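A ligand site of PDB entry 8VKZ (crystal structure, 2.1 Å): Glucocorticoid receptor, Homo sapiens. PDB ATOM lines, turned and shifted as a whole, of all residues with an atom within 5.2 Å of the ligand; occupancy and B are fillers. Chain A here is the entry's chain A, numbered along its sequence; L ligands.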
ATOM      1  N   ILE A  34      29.286  -3.877 -16.612  1.00  0.00           N
ATOM      2  CA  ILE A  34      28.758  -5.153 -16.175  1.00  0.00           C
ATOM      3  C   ILE A  34      29.381  -5.585 -14.855  1.00  0.00           C
ATOM      4  O   ILE A  34      28.654  -5.888 -13.903  1.00  0.00           O
ATOM      5  CB  ILE A  34      28.938  -6.200 -17.316  1.00  0.00           C
ATOM      6  CG1 ILE A  34      27.826  -6.044 -18.366  1.00  0.00           C
ATOM      7  CG2 ILE A  34      28.972  -7.656 -16.801  1.00  0.00           C
ATOM      8  CD1 ILE A  34      26.410  -6.261 -17.813  1.00  0.00           C
ATOM      9  N   MET A  35      30.710  -5.515 -14.757  1.00  0.00           N
ATOM     10  CA  MET A  35      31.402  -5.965 -13.567  1.00  0.00           C
ATOM     11  C   MET A  35      31.210  -5.077 -12.349  1.00  0.00           C
ATOM     12  O   MET A  35      31.026  -5.612 -11.243  1.00  0.00           O
ATOM     13  CB  MET A  35      32.879  -6.195 -13.873  1.00  0.00           C
ATOM     14  CG  MET A  35      33.129  -7.641 -14.309  1.00  0.00           C
ATOM     15  SD  MET A  35      34.472  -7.787 -15.496  1.00  0.00           S
ATOM     16  CE  MET A  35      35.826  -7.100 -14.529  1.00  0.00           C
ATOM     17  N   LEU A  38      27.576  -5.516 -11.146  1.00  0.00           N
ATOM     18  CA  LEU A  38      27.467  -6.764 -10.439  1.00  0.00           C
ATOM     19  C   LEU A  38      28.082  -6.688  -9.051  1.00  0.00           C
ATOM     20  O   LEU A  38      27.530  -7.241  -8.117  1.00  0.00           O
ATOM     21  CB  LEU A  38      28.063  -7.900 -11.256  1.00  0.00           C
ATOM     22  CG  LEU A  38      27.207  -8.311 -12.443  1.00  0.00           C
ATOM     23  CD1 LEU A  38      27.941  -9.271 -13.332  1.00  0.00           C
ATOM     24  CD2 LEU A  38      25.894  -8.847 -11.999  1.00  0.00           C
ATOM     25  N   ASN A  39      29.204  -5.974  -8.907  1.00  0.00           N
ATOM     26  CA  ASN A  39      29.805  -5.755  -7.584  1.00  0.00           C
ATOM     27  C   ASN A  39      28.868  -4.933  -6.707  1.00  0.00           C
ATOM     28  O   ASN A  39      28.786  -5.193  -5.501  1.00  0.00           O
ATOM     29  CB  ASN A  39      31.137  -5.067  -7.692  1.00  0.00           C
ATOM     30  CG  ASN A  39      32.240  -5.996  -8.078  1.00  0.00           C
ATOM     31  OD1 ASN A  39      32.293  -7.136  -7.658  1.00  0.00           O
ATOM     32  ND2 ASN A  39      33.170  -5.510  -8.852  1.00  0.00           N
ATOM     33  N   LEU A  41      25.485  -4.937  -6.912  1.00  0.00           N
ATOM     34  CA  LEU A  41      24.423  -5.884  -6.610  1.00  0.00           C
ATOM     35  C   LEU A  41      24.914  -6.891  -5.548  1.00  0.00           C
ATOM     36  O   LEU A  41      24.226  -7.158  -4.571  1.00  0.00           O
ATOM     37  CB  LEU A  41      23.985  -6.567  -7.928  1.00  0.00           C
ATOM     38  CG  LEU A  41      22.985  -7.713  -7.828  1.00  0.00           C
ATOM     39  CD1 LEU A  41      21.672  -7.287  -7.163  1.00  0.00           C
ATOM     40  CD2 LEU A  41      22.784  -8.369  -9.193  1.00  0.00           C
ATOM     41  N   GLY A  42      26.143  -7.353  -5.674  1.00  0.00           N
ATOM     42  CA  GLY A  42      26.765  -8.243  -4.698  1.00  0.00           C
ATOM     43  C   GLY A  42      26.822  -7.626  -3.305  1.00  0.00           C
ATOM     44  O   GLY A  42      26.655  -8.314  -2.304  1.00  0.00           O
ATOM     45  N   GLN A  45      23.112  -7.794  -2.019  1.00  0.00           N
ATOM     46  CA  GLN A  45      22.838  -9.195  -1.735  1.00  0.00           C
ATOM     47  C   GLN A  45      23.576  -9.646  -0.475  1.00  0.00           C
ATOM     48  O   GLN A  45      23.046 -10.468   0.256  1.00  0.00           O
ATOM     49  CB  GLN A  45      23.309 -10.075  -2.898  1.00  0.00           C
ATOM     50  CG  GLN A  45      22.452 -10.013  -4.155  1.00  0.00           C
ATOM     51  CD  GLN A  45      23.018 -10.849  -5.295  1.00  0.00           C
ATOM     52  OE1 GLN A  45      24.117 -11.414  -5.207  1.00  0.00           O
ATOM     53  NE2 GLN A  45      22.287 -10.939  -6.388  1.00  0.00           N
ATOM     54  N   TRP A  75      30.847 -15.951   1.768  1.00  0.00           N
ATOM     55  CA  TRP A  75      30.040 -15.043   0.924  1.00  0.00           C
ATOM     56  C   TRP A  75      30.024 -15.401  -0.577  1.00  0.00           C
ATOM     57  O   TRP A  75      28.944 -15.478  -1.141  1.00  0.00           O
ATOM     58  CB  TRP A  75      30.420 -13.565   1.123  1.00  0.00           C
ATOM     59  CG  TRP A  75      31.693 -13.166   0.442  1.00  0.00           C
ATOM     60  CD1 TRP A  75      32.952 -13.393   0.884  1.00  0.00           C
ATOM     61  CD2 TRP A  75      31.810 -12.603  -0.866  1.00  0.00           C
ATOM     62  NE1 TRP A  75      33.870 -12.968  -0.053  1.00  0.00           N
ATOM     63  CE2 TRP A  75      33.180 -12.456  -1.130  1.00  0.00           C
ATOM     64  CE3 TRP A  75      30.891 -12.167  -1.820  1.00  0.00           C
ATOM     65  CZ2 TRP A  75      33.657 -11.889  -2.315  1.00  0.00           C
ATOM     66  CZ3 TRP A  75      31.364 -11.621  -3.003  1.00  0.00           C
ATOM     67  CH2 TRP A  75      32.721 -11.473  -3.236  1.00  0.00           C
ATOM     68  N   MET A  76      31.184 -15.693  -1.202  1.00  0.00           N
ATOM     69  CA  MET A  76      31.220 -16.057  -2.623  1.00  0.00           C
ATOM     70  C   MET A  76      30.478 -17.356  -2.894  1.00  0.00           C
ATOM     71  O   MET A  76      29.885 -17.509  -3.942  1.00  0.00           O
ATOM     72  CB  MET A  76      32.654 -16.129  -3.146  1.00  0.00           C
ATOM     73  CG  MET A  76      32.760 -16.440  -4.634  1.00  0.00           C
ATOM     74  SD  MET A  76      32.033 -15.162  -5.680  1.00  0.00           S
ATOM     75  CE  MET A  76      33.311 -13.988  -5.668  1.00  0.00           C
ATOM     76  N   MET A  79      26.666 -16.647  -2.844  1.00  0.00           N
ATOM     77  CA  MET A  79      26.383 -15.838  -4.020  1.00  0.00           C
ATOM     78  C   MET A  79      26.355 -16.641  -5.303  1.00  0.00           C
ATOM     79  O   MET A  79      25.435 -16.427  -6.112  1.00  0.00           O
ATOM     80  CB  MET A  79      27.420 -14.714  -4.169  1.00  0.00           C
ATOM     81  CG  MET A  79      27.449 -13.786  -3.000  1.00  0.00           C
ATOM     82  SD  MET A  79      25.890 -13.005  -2.539  1.00  0.00           S
ATOM     83  CE  MET A  79      26.539 -11.642  -1.800  1.00  0.00           C
ATOM     84  N   ALA A  80      27.343 -17.525  -5.520  1.00  0.00           N
ATOM     85  CA  ALA A  80      27.418 -18.382  -6.699  1.00  0.00           C
ATOM     86  C   ALA A  80      26.346 -19.479  -6.663  1.00  0.00           C
ATOM     87  O   ALA A  80      25.821 -19.873  -7.697  1.00  0.00           O
ATOM     88  CB  ALA A  80      28.821 -19.026  -6.809  1.00  0.00           C
ATOM     89  N   LEU A  83      23.047 -17.672  -7.362  1.00  0.00           N
ATOM     90  CA  LEU A  83      23.077 -17.348  -8.785  1.00  0.00           C
ATOM     91  C   LEU A  83      22.749 -18.624  -9.599  1.00  0.00           C
ATOM     92  O   LEU A  83      21.972 -18.547 -10.538  1.00  0.00           O
ATOM     93  CB  LEU A  83      24.443 -16.770  -9.174  1.00  0.00           C
ATOM     94  CG  LEU A  83      24.802 -16.731 -10.674  1.00  0.00           C
ATOM     95  CD1 LEU A  83      23.966 -15.737 -11.406  1.00  0.00           C
ATOM     96  CD2 LEU A  83      26.283 -16.434 -10.875  1.00  0.00           C
ATOM     97  N   ARG A  86      18.834 -19.447  -9.376  1.00  0.00           N
ATOM     98  CA  ARG A  86      18.075 -18.507 -10.184  1.00  0.00           C
ATOM     99  C   ARG A  86      18.218 -18.786 -11.687  1.00  0.00           C
ATOM    100  O   ARG A  86      17.265 -18.629 -12.449  1.00  0.00           O
ATOM    101  CB  ARG A  86      18.535 -17.063  -9.863  1.00  0.00           C
ATOM    102  CG  ARG A  86      18.090 -16.592  -8.466  1.00  0.00           C
ATOM    103  CD  ARG A  86      18.203 -15.084  -8.245  1.00  0.00           C
ATOM    104  NE  ARG A  86      19.496 -14.555  -8.668  1.00  0.00           N
ATOM    105  CZ  ARG A  86      20.558 -14.450  -7.875  1.00  0.00           C
ATOM    106  NH1 ARG A  86      20.481 -14.781  -6.591  1.00  0.00           N
ATOM    107  NH2 ARG A  86      21.708 -13.999  -8.367  1.00  0.00           N
ATOM    108  N   LEU A  96      22.844 -16.896 -17.135  1.00  0.00           N
ATOM    109  CA  LEU A  96      23.303 -16.531 -15.805  1.00  0.00           C
ATOM    110  C   LEU A  96      22.346 -15.435 -15.308  1.00  0.00           C
ATOM    111  O   LEU A  96      22.456 -14.275 -15.684  1.00  0.00           O
ATOM    112  CB  LEU A  96      24.746 -16.005 -15.818  1.00  0.00           C
ATOM    113  CG  LEU A  96      25.880 -17.010 -16.016  1.00  0.00           C
ATOM    114  CD1 LEU A  96      27.223 -16.310 -15.955  1.00  0.00           C
ATOM    115  CD2 LEU A  96      25.820 -18.117 -14.973  1.00  0.00           C
ATOM    116  N   PHE A  98      21.737 -13.208 -12.856  1.00  0.00           N
ATOM    117  CA  PHE A  98      22.287 -12.396 -11.766  1.00  0.00           C
ATOM    118  C   PHE A  98      21.175 -11.653 -11.078  1.00  0.00           C
ATOM    119  O   PHE A  98      21.068 -11.664  -9.858  1.00  0.00           O
ATOM    120  CB  PHE A  98      23.329 -11.414 -12.322  1.00  0.00           C
ATOM    121  CG  PHE A  98      24.608 -12.108 -12.686  1.00  0.00           C
ATOM    122  CD1 PHE A  98      25.546 -12.417 -11.716  1.00  0.00           C
ATOM    123  CD2 PHE A  98      24.875 -12.457 -14.002  1.00  0.00           C
ATOM    124  CE1 PHE A  98      26.739 -13.043 -12.066  1.00  0.00           C
ATOM    125  CE2 PHE A  98      26.066 -13.067 -14.333  1.00  0.00           C
ATOM    126  CZ  PHE A  98      26.988 -13.365 -13.364  1.00  0.00           C
ATOM    127  N   ILE A 104      22.680 -12.548 -18.093  1.00  0.00           N
ATOM    128  CA  ILE A 104      23.728 -12.735 -19.080  1.00  0.00           C
ATOM    129  C   ILE A 104      23.427 -13.990 -19.867  1.00  0.00           C
ATOM    130  O   ILE A 104      23.557 -15.103 -19.350  1.00  0.00           O
ATOM    131  CB  ILE A 104      25.163 -12.749 -18.483  1.00  0.00           C
ATOM    132  CG1 ILE A 104      25.438 -11.534 -17.570  1.00  0.00           C
ATOM    133  CG2 ILE A 104      26.192 -12.873 -19.596  1.00  0.00           C
ATOM    134  CD1 ILE A 104      25.545 -10.206 -18.255  1.00  0.00           C
ATOM    135  N   GLU A 106      24.742 -16.355 -22.017  1.00  0.00           N
ATOM    136  CA  GLU A 106      26.086 -16.874 -22.300  1.00  0.00           C
ATOM    137  C   GLU A 106      26.574 -16.611 -23.735  1.00  0.00           C
ATOM    138  O   GLU A 106      27.753 -16.348 -23.937  1.00  0.00           O
ATOM    139  CB  GLU A 106      26.173 -18.388 -21.921  1.00  0.00           C
ATOM    140  CG  GLU A 106      27.215 -19.257 -22.624  1.00  0.00           C
ATOM    141  CD  GLU A 106      28.661 -19.119 -22.164  1.00  0.00           C
ATOM    142  OE1 GLU A 106      29.314 -20.163 -21.956  1.00  0.00           O
ATOM    143  OE2 GLU A 106      29.139 -17.965 -22.043  1.00  0.00           O
ATOM    144  N   MET A 114      36.342 -13.712 -19.524  1.00  0.00           N
ATOM    145  CA  MET A 114      35.652 -14.421 -18.450  1.00  0.00           C
ATOM    146  C   MET A 114      35.210 -15.818 -18.888  1.00  0.00           C
ATOM    147  O   MET A 114      34.125 -16.259 -18.519  1.00  0.00           O
ATOM    148  CB  MET A 114      34.475 -13.595 -17.921  1.00  0.00           C
ATOM    149  CG  MET A 114      34.891 -12.429 -17.037  1.00  0.00           C
ATOM    150  SD  MET A 114      35.572 -10.950 -17.869  1.00  0.00           S
ATOM    151  CE  MET A 114      34.271 -10.587 -19.019  1.00  0.00           C
ATOM    152  N   GLN A 117      35.850 -18.056 -15.758  1.00  0.00           N
ATOM    153  CA  GLN A 117      34.872 -17.594 -14.782  1.00  0.00           C
ATOM    154  C   GLN A 117      33.452 -18.052 -15.108  1.00  0.00           C
ATOM    155  O   GLN A 117      32.837 -18.748 -14.289  1.00  0.00           O
ATOM    156  CB  GLN A 117      34.921 -16.060 -14.643  1.00  0.00           C
ATOM    157  CG  GLN A 117      36.083 -15.572 -13.822  1.00  0.00           C
ATOM    158  CD  GLN A 117      37.388 -15.842 -14.493  1.00  0.00           C
ATOM    159  OE1 GLN A 117      37.579 -15.536 -15.675  1.00  0.00           O
ATOM    160  NE2 GLN A 117      38.309 -16.459 -13.762  1.00  0.00           N
ATOM    161  N   CYS A 118      32.950 -17.700 -16.312  1.00  0.00           N
ATOM    162  CA  CYS A 118      31.611 -18.045 -16.773  1.00  0.00           C
ATOM    163  C   CYS A 118      31.349 -19.549 -16.740  1.00  0.00           C
ATOM    164  O   CYS A 118      30.237 -19.961 -16.403  1.00  0.00           O
ATOM    165  CB  CYS A 118      31.358 -17.462 -18.157  1.00  0.00           C
ATOM    166  SG  CYS A 118      29.666 -17.722 -18.780  1.00  0.00           S
ATOM    167  N   MET A 121      30.553 -20.496 -13.165  1.00  0.00           N
ATOM    168  CA  MET A 121      29.245 -20.002 -12.759  1.00  0.00           C
ATOM    169  C   MET A 121      28.156 -20.874 -13.370  1.00  0.00           C
ATOM    170  O   MET A 121      27.209 -21.256 -12.677  1.00  0.00           O
ATOM    171  CB  MET A 121      29.073 -18.554 -13.170  1.00  0.00           C
ATOM    172  CG  MET A 121      29.679 -17.610 -12.195  1.00  0.00           C
ATOM    173  SD  MET A 121      29.948 -16.023 -12.951  1.00  0.00           S
ATOM    174  CE  MET A 121      30.667 -15.202 -11.653  1.00  0.00           C
ATOM    175  N   LEU A 207      36.341 -18.116  -8.832  1.00  0.00           N
ATOM    176  CA  LEU A 207      35.628 -16.833  -8.802  1.00  0.00           C
ATOM    177  C   LEU A 207      36.262 -15.835  -7.823  1.00  0.00           C
ATOM    178  O   LEU A 207      36.329 -14.645  -8.131  1.00  0.00           O
ATOM    179  CB  LEU A 207      34.129 -17.029  -8.501  1.00  0.00           C
ATOM    180  CG  LEU A 207      33.378 -18.041  -9.385  1.00  0.00           C
ATOM    181  CD1 LEU A 207      31.939 -18.167  -8.972  1.00  0.00           C
ATOM    182  CD2 LEU A 207      33.482 -17.690 -10.852  1.00  0.00           C
ATOM    183  N   TYR A 210      39.429 -14.402  -9.414  1.00  0.00           N
ATOM    184  CA  TYR A 210      39.140 -13.334 -10.366  1.00  0.00           C
ATOM    185  C   TYR A 210      38.682 -12.077  -9.665  1.00  0.00           C
ATOM    186  O   TYR A 210      38.969 -10.970 -10.099  1.00  0.00           O
ATOM    187  CB  TYR A 210      38.070 -13.749 -11.367  1.00  0.00           C
ATOM    188  CG  TYR A 210      37.987 -12.774 -12.525  1.00  0.00           C
ATOM    189  CD1 TYR A 210      39.056 -12.610 -13.397  1.00  0.00           C
ATOM    190  CD2 TYR A 210      36.861 -11.988 -12.726  1.00  0.00           C
ATOM    191  CE1 TYR A 210      38.994 -11.716 -14.456  1.00  0.00           C
ATOM    192  CE2 TYR A 210      36.785 -11.095 -13.774  1.00  0.00           C
ATOM    193  CZ  TYR A 210      37.858 -10.958 -14.645  1.00  0.00           C
ATOM    194  OH  TYR A 210      37.812 -10.076 -15.702  1.00  0.00           O
ATOM    195  N   CYS A 211      37.962 -12.243  -8.577  1.00  0.00           N
ATOM    196  CA  CYS A 211      37.486 -11.149  -7.768  1.00  0.00           C
ATOM    197  C   CYS A 211      38.694 -10.370  -7.180  1.00  0.00           C
ATOM    198  O   CYS A 211      38.775  -9.149  -7.340  1.00  0.00           O
ATOM    199  CB  CYS A 211      36.576 -11.700  -6.677  1.00  0.00           C
ATOM    200  SG  CYS A 211      36.063 -10.490  -5.456  1.00  0.00           S
ATOM    201  N   THR A 214      40.474  -8.260  -9.961  1.00  0.00           N
ATOM    202  CA  THR A 214      39.790  -7.020 -10.320  1.00  0.00           C
ATOM    203  C   THR A 214      39.752  -6.017  -9.158  1.00  0.00           C
ATOM    204  O   THR A 214      39.704  -4.804  -9.375  1.00  0.00           O
ATOM    205  CB  THR A 214      38.404  -7.321 -10.905  1.00  0.00           C
ATOM    206  OG1 THR A 214      37.531  -7.794  -9.873  1.00  0.00           O
ATOM    207  CG2 THR A 214      38.464  -8.330 -12.077  1.00  0.00           C
ATOM    208  N   ILE A 222      37.859  -1.329 -11.556  1.00  0.00           N
ATOM    209  CA  ILE A 222      36.484  -1.767 -11.333  1.00  0.00           C
ATOM    210  C   ILE A 222      36.078  -1.312  -9.924  1.00  0.00           C
ATOM    211  O   ILE A 222      36.874  -1.431  -9.002  1.00  0.00           O
ATOM    212  CB  ILE A 222      36.400  -3.316 -11.499  1.00  0.00           C
ATOM    213  CG1 ILE A 222      36.709  -3.752 -12.938  1.00  0.00           C
ATOM    214  CG2 ILE A 222      35.063  -3.884 -11.051  1.00  0.00           C
ATOM    215  CD1 ILE A 222      35.869  -3.119 -13.964  1.00  0.00           C
ATOM    216  N   PHE A 224      33.718  -1.291  -6.361  1.00  0.00           N
ATOM    217  CA  PHE A 224      33.089  -2.228  -5.425  1.00  0.00           C
ATOM    218  C   PHE A 224      32.460  -1.413  -4.332  1.00  0.00           C
ATOM    219  O   PHE A 224      33.037  -0.434  -3.883  1.00  0.00           O
ATOM    220  CB  PHE A 224      34.153  -3.122  -4.728  1.00  0.00           C
ATOM    221  CG  PHE A 224      34.857  -4.166  -5.557  1.00  0.00           C
ATOM    222  CD1 PHE A 224      35.894  -3.809  -6.399  1.00  0.00           C
ATOM    223  CD2 PHE A 224      34.534  -5.511  -5.439  1.00  0.00           C
ATOM    224  CE1 PHE A 224      36.516  -4.758  -7.186  1.00  0.00           C
ATOM    225  CE2 PHE A 224      35.200  -6.466  -6.196  1.00  0.00           C
ATOM    226  CZ  PHE A 224      36.177  -6.091  -7.069  1.00  0.00           C
ATOM    227  N   LEU A 228      31.562  -5.181   0.267  1.00  0.00           N
ATOM    228  CA  LEU A 228      32.434  -6.154  -0.382  1.00  0.00           C
ATOM    229  C   LEU A 228      33.895  -5.792  -0.277  1.00  0.00           C
ATOM    230  O   LEU A 228      34.714  -6.687  -0.088  1.00  0.00           O
ATOM    231  CB  LEU A 228      32.053  -6.342  -1.843  1.00  0.00           C
ATOM    232  CG  LEU A 228      30.754  -7.054  -2.145  1.00  0.00           C
ATOM    233  CD1 LEU A 228      30.713  -7.441  -3.622  1.00  0.00           C
ATOM    234  CD2 LEU A 228      30.560  -8.317  -1.264  1.00  0.00           C
HETATM  235  C1  LIG L   1      29.425 -11.442  -8.375  1.00  0.00           C
HETATM  236  C2  LIG L   1      30.540 -12.499  -8.285  1.00  0.00           C
HETATM  237  C3  LIG L   1      29.972 -13.914  -8.517  1.00  0.00           C
HETATM  238  C4  LIG L   1      28.758 -14.220  -7.646  1.00  0.00           C
HETATM  239  C5  LIG L   1      27.750 -13.101  -7.694  1.00  0.00           C
HETATM  240  C6  LIG L   1      25.517 -12.225  -8.196  1.00  0.00           C
HETATM  241  C7  LIG L   1      28.278 -11.729  -7.336  1.00  0.00           C
HETATM  242  C8  LIG L   1      31.589 -12.179  -9.365  1.00  0.00           C
HETATM  243  C9  LIG L   1      33.711 -12.319 -10.488  1.00  0.00           C
HETATM  244  C10 LIG L   1      34.358  -9.815 -10.372  1.00  0.00           C
HETATM  245  C11 LIG L   1      34.035  -8.400 -10.756  1.00  0.00           C
HETATM  246  C12 LIG L   1      32.167 -11.879 -13.702  1.00  0.00           C
HETATM  247  C13 LIG L   1      31.505 -13.266 -15.565  1.00  0.00           C
HETATM  248  C14 LIG L   1      29.303 -12.951 -16.752  1.00  0.00           C
HETATM  249  C15 LIG L   1      30.528 -11.990 -18.748  1.00  0.00           C
HETATM  250  C16 LIG L   1      31.118 -12.124 -19.992  1.00  0.00           C
HETATM  251  C17 LIG L   1      30.978 -11.187 -13.833  1.00  0.00           C
HETATM  252  C18 LIG L   1      32.420 -12.924 -14.583  1.00  0.00           C
HETATM  253  C19 LIG L   1      30.069 -11.520 -14.816  1.00  0.00           C
HETATM  254  C20 LIG L   1      31.049 -13.330 -20.678  1.00  0.00           C
HETATM  255  C21 LIG L   1      29.823 -14.270 -18.836  1.00  0.00           C
HETATM  256  C22 LIG L   1      30.314 -12.560 -15.696  1.00  0.00           C
HETATM  257  C23 LIG L   1      29.892 -13.063 -18.139  1.00  0.00           C
HETATM  258  C24 LIG L   1      30.378 -14.418 -20.108  1.00  0.00           C
HETATM  259  C25 LIG L   1      25.971 -10.885  -7.843  1.00  0.00           C
HETATM  260  C26 LIG L   1      26.492 -13.302  -8.111  1.00  0.00           C
HETATM  261  C27 LIG L   1      27.218 -10.666  -7.448  1.00  0.00           C
HETATM  262  C28 LIG L   1      32.780 -13.127  -9.570  1.00  0.00           C
HETATM  263  C29 LIG L   1      31.128  -9.734  -9.322  1.00  0.00           C
HETATM  264  C30 LIG L   1      33.130 -11.547 -12.600  1.00  0.00           C
HETATM  265  C31 LIG L   1      29.958  -9.975  -8.359  1.00  0.00           C
HETATM  266  C32 LIG L   1      33.231 -10.844 -10.433  1.00  0.00           C
HETATM  267  C33 LIG L   1      32.243 -10.791  -9.222  1.00  0.00           C
HETATM  268  C34 LIG L   1      28.751 -11.749  -5.855  1.00  0.00           C
HETATM  269  C35 LIG L   1      33.045 -10.640  -7.916  1.00  0.00           C
HETATM  270  N1  LIG L   1      30.228 -15.601 -20.805  1.00  0.00           N
HETATM  271  O1  LIG L   1      24.337 -12.447  -8.502  1.00  0.00           O
HETATM  272  O2  LIG L   1      35.486 -10.108 -10.051  1.00  0.00           O
HETATM  273  O3  LIG L   1      33.441 -12.719 -11.848  1.00  0.00           O
HETATM  274  O4  LIG L   1      32.531 -10.672 -11.664  1.00  0.00           O
HETATM  275  O5  LIG L   1      30.246  -9.458  -7.061  1.00  0.00           O
HETATM  276  O6  LIG L   1      35.061  -7.499 -10.409  1.00  0.00           O
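The side-chain hydroxyl (OG1) of Thr 214 sits at hydrogen-bond distance from the backbone carbonyl oxygen (O) of Cys 211 (3.1 Å).
The backbone carbonyl oxygen of Tyr 210 sits close to the side-chain hydroxyl of Thr 214, 3.5 Å away.
The side-chain sulfur (SG) of Cys 118 lies within hydrogen-bond range of the side-chain carboxylate (OE2) of Glu 106 (3.3 Å).
The guanidinium group of Arg 86 sits at hydrogen-bond distance from the backbone carbonyl oxygen of Phe 98, at 2.8 Å.
The side-chain amide nitrogen (ND2) of Asn 39 sits at hydrogen-bond distance from the backbone carbonyl oxygen (O) of Met 35, 3.2 Å away.
The side-chain sulfur (SD) of Met 79 sits close to the side-chain amide oxygen (OE1) of Gln 45 (3.6 Å).
The side-chain hydroxyl of Tyr 210 lies within hydrogen-bond range of the side-chain sulfur of Met 114.
O of Ile 104 is in hydrogen-bond range of N of Leu 96 (2.9 Å).
An oxygen (O6) of the ligand sits at hydrogen-bond distance from the side-chain hydroxyl of Thr 214, at 2.5 Å.
The side-chain carboxylate of Glu 106 is in hydrogen-bond range of a nitrogen (N1) of the ligand, at 2.9 Å.
SG of Cys 118 lies within hydrogen-bond range of N1 of the ligand (3.0 Å).
An oxygen (O1) of the ligand lies within hydrogen-bond range of the guanidinium group (NH2) of Arg 86, 3.1 Å away.
OD1 of Asn 39 lies within hydrogen-bond range of O5 of the ligand, 3.2 Å away.
O1 of the ligand sits at hydrogen-bond distance from NE2 of Gln 45.
Met 35 touches the ligand.
Leu 38 touches the ligand (CD1 to C19, 3.4 Å).
CA of Gly 42 touches C27 of the ligand, 3.7 Å away.
CZ3 of Trp 75 touches C34 of the ligand, 3.9 Å away.
Met 76 touches the ligand (SD to C3, 3.7 Å).
Met 79 touches the ligand (CB to C34, 3.7 Å).
Phe 98 touches the ligand.
CG2 of Ile 104 touches C21 of the ligand, 3.96 Å away.
Met 114 touches the ligand.
CE of Met 121 touches C3 of the ligand (3.5 Å).
Tyr 210 touches the ligand.
Cys 211 touches the ligand (CA to O2, 3.2 Å).
Ile 222 touches the ligand.
Phe 224 touches the ligand.
Hydrophobic or aromatic side chains within 4 Å of the ligand: Met 35, Leu 38, Trp 75, Met 76, Met 79, Phe 98, Ile 104, Met 114, Met 121, Tyr 210, Ile 222 and Phe 224.
20 residues have an atom within 4 Å of the ligand: Met 35, Leu 38, Asn 39, Gly 42, Gln 45, Trp 75, Met 76, Met 79, Arg 86, Phe 98, Ile 104, Glu 106, Met 114, Cys 118, Met 121, Tyr 210, Cys 211, Thr 214, Ile 222 and Phe 224.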
